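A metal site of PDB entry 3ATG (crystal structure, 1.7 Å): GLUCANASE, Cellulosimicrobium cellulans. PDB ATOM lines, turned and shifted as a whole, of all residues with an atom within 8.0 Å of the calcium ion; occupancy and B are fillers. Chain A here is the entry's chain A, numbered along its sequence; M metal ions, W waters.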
ATOM      1  N   ASP A   9     -27.003 -29.340  -5.017  1.00  0.00           N
ATOM      2  CA  ASP A   9     -27.415 -28.045  -5.521  1.00  0.00           C
ATOM      3  C   ASP A   9     -26.135 -27.223  -5.661  1.00  0.00           C
ATOM      4  O   ASP A   9     -25.437 -26.956  -4.668  1.00  0.00           O
ATOM      5  CB  ASP A   9     -28.423 -27.364  -4.591  1.00  0.00           C
ATOM      6  CG  ASP A   9     -29.068 -26.152  -5.234  1.00  0.00           C
ATOM      7  OD1 ASP A   9     -28.498 -25.664  -6.237  1.00  0.00           O
ATOM      8  OD2 ASP A   9     -30.112 -25.674  -4.734  1.00  0.00           O
ATOM      9  N   GLU A  10     -25.775 -26.870  -6.894  1.00  0.00           N
ATOM     10  CA  GLU A  10     -24.571 -26.080  -7.148  1.00  0.00           C
ATOM     11  C   GLU A  10     -24.829 -24.577  -7.199  1.00  0.00           C
ATOM     12  O   GLU A  10     -23.906 -23.788  -7.362  1.00  0.00           O
ATOM     13  CB  GLU A  10     -23.892 -26.537  -8.459  1.00  0.00           C
ATOM     14  CG  GLU A  10     -23.634 -28.056  -8.540  1.00  0.00           C
ATOM     15  CD  GLU A  10     -22.512 -28.549  -7.637  1.00  0.00           C
ATOM     16  OE1 GLU A  10     -22.525 -29.739  -7.291  1.00  0.00           O
ATOM     17  OE2 GLU A  10     -21.601 -27.761  -7.314  1.00  0.00           O
ATOM     18  N   PHE A  11     -26.090 -24.186  -7.025  1.00  0.00           N
ATOM     19  CA  PHE A  11     -26.498 -22.773  -7.000  1.00  0.00           C
ATOM     20  C   PHE A  11     -26.098 -22.028  -8.257  1.00  0.00           C
ATOM     21  O   PHE A  11     -25.634 -20.880  -8.210  1.00  0.00           O
ATOM     22  CB  PHE A  11     -26.028 -22.084  -5.716  1.00  0.00           C
ATOM     23  CG  PHE A  11     -26.554 -22.751  -4.487  1.00  0.00           C
ATOM     24  CD1 PHE A  11     -25.704 -23.446  -3.623  1.00  0.00           C
ATOM     25  CD2 PHE A  11     -27.916 -22.717  -4.202  1.00  0.00           C
ATOM     26  CE1 PHE A  11     -26.206 -24.081  -2.486  1.00  0.00           C
ATOM     27  CE2 PHE A  11     -28.425 -23.364  -3.069  1.00  0.00           C
ATOM     28  CZ  PHE A  11     -27.565 -24.045  -2.210  1.00  0.00           C
ATOM     29  N   ASP A  12     -26.311 -22.683  -9.397  1.00  0.00           N
ATOM     30  CA  ASP A  12     -26.079 -22.052 -10.685  1.00  0.00           C
ATOM     31  C   ASP A  12     -27.227 -21.104 -10.967  1.00  0.00           C
ATOM     32  O   ASP A  12     -28.376 -21.361 -10.594  1.00  0.00           O
ATOM     33  CB  ASP A  12     -26.070 -23.098 -11.800  1.00  0.00           C
ATOM     34  CG  ASP A  12     -24.906 -24.083 -11.693  1.00  0.00           C
ATOM     35  OD1 ASP A  12     -25.072 -25.226 -12.167  1.00  0.00           O
ATOM     36  OD2 ASP A  12     -23.836 -23.703 -11.198  1.00  0.00           O
ATOM     37  N   GLY A  13     -26.920 -20.017 -11.659  1.00  0.00           N
ATOM     38  CA  GLY A  13     -27.975 -19.087 -12.035  1.00  0.00           C
ATOM     39  C   GLY A  13     -27.477 -17.651 -12.060  1.00  0.00           C
ATOM     40  O   GLY A  13     -26.424 -17.322 -11.527  1.00  0.00           O
ATOM     41  N   ASP A  51     -26.007 -15.251  -6.517  1.00  0.00           N
ATOM     42  CA  ASP A  51     -25.176 -14.080  -6.819  1.00  0.00           C
ATOM     43  C   ASP A  51     -24.632 -14.011  -8.247  1.00  0.00           C
ATOM     44  O   ASP A  51     -23.974 -13.022  -8.608  1.00  0.00           O
ATOM     45  CB  ASP A  51     -24.048 -13.927  -5.785  1.00  0.00           C
ATOM     46  CG  ASP A  51     -22.988 -15.024  -5.882  1.00  0.00           C
ATOM     47  OD1 ASP A  51     -23.132 -15.942  -6.713  1.00  0.00           O
ATOM     48  OD2 ASP A  51     -22.003 -14.948  -5.109  1.00  0.00           O
ATOM     49  N   GLN A  53     -22.424 -15.823  -9.414  1.00  0.00           N
ATOM     50  CA  GLN A  53     -21.075 -16.373  -9.377  1.00  0.00           C
ATOM     51  C   GLN A  53     -21.090 -17.837  -8.893  1.00  0.00           C
ATOM     52  O   GLN A  53     -20.050 -18.416  -8.588  1.00  0.00           O
ATOM     53  CB  GLN A  53     -20.184 -15.537  -8.452  1.00  0.00           C
ATOM     54  CG  GLN A  53     -20.027 -14.096  -8.911  1.00  0.00           C
ATOM     55  CD  GLN A  53     -19.342 -14.010 -10.253  1.00  0.00           C
ATOM     56  OE1 GLN A  53     -18.312 -14.643 -10.485  1.00  0.00           O
ATOM     57  NE2 GLN A  53     -19.922 -13.230 -11.171  1.00  0.00           N
ATOM     58  N   GLY A  54     -22.283 -18.422  -8.844  1.00  0.00           N
ATOM     59  CA  GLY A  54     -22.421 -19.811  -8.430  1.00  0.00           C
ATOM     60  C   GLY A  54     -22.646 -19.982  -6.947  1.00  0.00           C
ATOM     61  O   GLY A  54     -22.437 -21.076  -6.431  1.00  0.00           O
ATOM     62  N   ASN A  55     -23.063 -18.934  -6.254  1.00  0.00           N
ATOM     63  CA  ASN A  55     -23.334 -19.044  -4.812  1.00  0.00           C
ATOM     64  C   ASN A  55     -24.753 -18.660  -4.461  1.00  0.00           C
ATOM     65  O   ASN A  55     -25.293 -17.706  -5.017  1.00  0.00           O
ATOM     66  CB  ASN A  55     -22.419 -18.121  -3.998  1.00  0.00           C
ATOM     67  CG  ASN A  55     -20.947 -18.350  -4.299  1.00  0.00           C
ATOM     68  OD1 ASN A  55     -20.447 -19.467  -4.175  1.00  0.00           O
ATOM     69  ND2 ASN A  55     -20.254 -17.291  -4.729  1.00  0.00           N
ATOM     70  N   LEU A  56     -25.341 -19.397  -3.521  1.00  0.00           N
ATOM     71  CA  LEU A  56     -26.470 -18.913  -2.745  1.00  0.00           C
ATOM     72  C   LEU A  56     -25.945 -17.879  -1.759  1.00  0.00           C
ATOM     73  O   LEU A  56     -24.903 -18.084  -1.142  1.00  0.00           O
ATOM     74  CB  LEU A  56     -27.113 -20.076  -1.995  1.00  0.00           C
ATOM     75  CG  LEU A  56     -28.135 -19.693  -0.915  1.00  0.00           C
ATOM     76  CD1 LEU A  56     -29.417 -19.143  -1.551  1.00  0.00           C
ATOM     77  CD2 LEU A  56     -28.436 -20.883   0.000  1.00  0.00           C
ATOM     78  N   ARG A  89     -19.979 -26.154   0.928  1.00  0.00           N
ATOM     79  CA  ARG A  89     -18.856 -25.243   0.893  1.00  0.00           C
ATOM     80  C   ARG A  89     -19.396 -23.851   1.184  1.00  0.00           C
ATOM     81  O   ARG A  89     -20.193 -23.308   0.406  1.00  0.00           O
ATOM     82  CB  ARG A  89     -18.178 -25.296  -0.483  1.00  0.00           C
ATOM     83  CG  ARG A  89     -16.974 -24.397  -0.606  1.00  0.00           C
ATOM     84  CD  ARG A  89     -16.150 -24.730  -1.847  1.00  0.00           C
ATOM     85  NE  ARG A  89     -14.914 -23.950  -1.860  1.00  0.00           N
ATOM     86  CZ  ARG A  89     -14.714 -22.880  -2.607  1.00  0.00           C
ATOM     87  NH1 ARG A  89     -15.666 -22.474  -3.450  1.00  0.00           N
ATOM     88  NH2 ARG A  89     -13.556 -22.221  -2.532  1.00  0.00           N
ATOM     89  N   PHE A 164     -14.208 -19.381   1.687  1.00  0.00           N
ATOM     90  CA  PHE A 164     -15.014 -20.600   1.718  1.00  0.00           C
ATOM     91  C   PHE A 164     -14.283 -21.744   2.401  1.00  0.00           C
ATOM     92  O   PHE A 164     -13.087 -21.960   2.175  1.00  0.00           O
ATOM     93  CB  PHE A 164     -15.373 -21.051   0.297  1.00  0.00           C
ATOM     94  CG  PHE A 164     -16.355 -20.160  -0.409  1.00  0.00           C
ATOM     95  CD1 PHE A 164     -17.709 -20.436  -0.385  1.00  0.00           C
ATOM     96  CD2 PHE A 164     -15.906 -19.056  -1.121  1.00  0.00           C
ATOM     97  CE1 PHE A 164     -18.613 -19.603  -1.051  1.00  0.00           C
ATOM     98  CE2 PHE A 164     -16.789 -18.230  -1.782  1.00  0.00           C
ATOM     99  CZ  PHE A 164     -18.148 -18.499  -1.748  1.00  0.00           C
ATOM    100  N   VAL A 232     -22.966 -19.729  -0.036  1.00  0.00           N
ATOM    101  CA  VAL A 232     -22.892 -21.185  -0.121  1.00  0.00           C
ATOM    102  C   VAL A 232     -22.638 -21.570  -1.577  1.00  0.00           C
ATOM    103  O   VAL A 232     -23.472 -21.316  -2.444  1.00  0.00           O
ATOM    104  CB  VAL A 232     -24.182 -21.849   0.373  1.00  0.00           C
ATOM    105  CG1 VAL A 232     -24.011 -23.372   0.405  1.00  0.00           C
ATOM    106  CG2 VAL A 232     -24.591 -21.312   1.768  1.00  0.00           C
ATOM    107  N   ASP A 233     -21.475 -22.155  -1.846  1.00  0.00           N
ATOM    108  CA  ASP A 233     -21.085 -22.537  -3.199  1.00  0.00           C
ATOM    109  C   ASP A 233     -21.837 -23.792  -3.640  1.00  0.00           C
ATOM    110  O   ASP A 233     -22.247 -23.929  -4.799  1.00  0.00           O
ATOM    111  CB  ASP A 233     -19.574 -22.773  -3.213  1.00  0.00           C
ATOM    112  CG  ASP A 233     -19.024 -23.115  -4.587  1.00  0.00           C
ATOM    113  OD1 ASP A 233     -19.672 -22.840  -5.620  1.00  0.00           O
ATOM    114  OD2 ASP A 233     -17.892 -23.643  -4.637  1.00  0.00           O
ATOM    115  N   TYR A 234     -22.038 -24.739  -2.726  1.00  0.00           N
ATOM    116  CA  TYR A 234     -22.764 -25.948  -3.064  1.00  0.00           C
ATOM    117  C   TYR A 234     -23.212 -26.660  -1.802  1.00  0.00           C
ATOM    118  O   TYR A 234     -22.681 -26.436  -0.727  1.00  0.00           O
ATOM    119  CB  TYR A 234     -21.910 -26.928  -3.905  1.00  0.00           C
ATOM    120  CG  TYR A 234     -20.619 -27.422  -3.285  1.00  0.00           C
ATOM    121  CD1 TYR A 234     -19.381 -27.023  -3.792  1.00  0.00           C
ATOM    122  CD2 TYR A 234     -20.633 -28.334  -2.236  1.00  0.00           C
ATOM    123  CE1 TYR A 234     -18.198 -27.491  -3.239  1.00  0.00           C
ATOM    124  CE2 TYR A 234     -19.434 -28.802  -1.668  1.00  0.00           C
ATOM    125  CZ  TYR A 234     -18.232 -28.382  -2.201  1.00  0.00           C
ATOM    126  OH  TYR A 234     -17.047 -28.827  -1.663  1.00  0.00           O
ATOM    127  N   VAL A 235     -24.233 -27.498  -1.955  1.00  0.00           N
ATOM    128  CA  VAL A 235     -24.580 -28.521  -0.982  1.00  0.00           C
ATOM    129  C   VAL A 235     -24.546 -29.829  -1.779  1.00  0.00           C
ATOM    130  O   VAL A 235     -25.193 -29.933  -2.826  1.00  0.00           O
ATOM    131  CB  VAL A 235     -25.969 -28.307  -0.364  1.00  0.00           C
ATOM    132  CG1 VAL A 235     -26.334 -29.476   0.548  1.00  0.00           C
ATOM    133  CG2 VAL A 235     -26.002 -26.992   0.393  1.00  0.00           C
ATOM    134  N   ARG A 236     -23.768 -30.801  -1.309  1.00  0.00           N
ATOM    135  CA  ARG A 236     -23.579 -32.065  -2.041  1.00  0.00           C
ATOM    136  C   ARG A 236     -23.766 -33.272  -1.152  1.00  0.00           C
ATOM    137  O   ARG A 236     -23.486 -33.204   0.039  1.00  0.00           O
ATOM    138  CB  ARG A 236     -22.167 -32.128  -2.618  1.00  0.00           C
ATOM    139  CG  ARG A 236     -21.933 -31.181  -3.778  1.00  0.00           C
ATOM    140  CD  ARG A 236     -20.526 -31.304  -4.317  1.00  0.00           C
ATOM    141  NE  ARG A 236     -20.305 -30.326  -5.378  1.00  0.00           N
ATOM    142  CZ  ARG A 236     -19.113 -29.929  -5.802  1.00  0.00           C
ATOM    143  NH1 ARG A 236     -18.020 -30.458  -5.278  1.00  0.00           N
ATOM    144  NH2 ARG A 236     -19.017 -28.993  -6.749  1.00  0.00           N
HETATM  145 CA    CA M   1     -21.607 -23.207  -7.038  1.00  0.00          CA
HETATM  146  O   HOH W   1     -19.650 -22.226  -8.313  1.00  0.00           O
HETATM  147  O   HOH W   2     -20.645 -25.375  -7.445  1.00  0.00           O
HETATM  148  O   HOH W   3     -22.008 -23.016  -9.437  1.00  0.00           O
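Within 4 Å of the calcium ion: Glu 10, Gly 54 and Asp 233.
The backbone NH of Gly 54 is in hydrogen-bond range of the side-chain carboxylate of Asp 51 (3.4 Å). OE2 of Glu 10 is in salt-bridge range of NH2 of Arg 236. OD2 of Asp 233 is in salt-bridge range of NH1 of Arg 89 (2.8 Å).
The calcium ion is bound by O of Gly 54 (2.4 Å), O of Glu 10 (2.4 Å), water W2 (2.4 Å), OD1 of Asp 233 (2.4 Å), O of Asp 233 (2.4 Å), water W3 (2.4 Å) and water W1 (2.5 Å).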
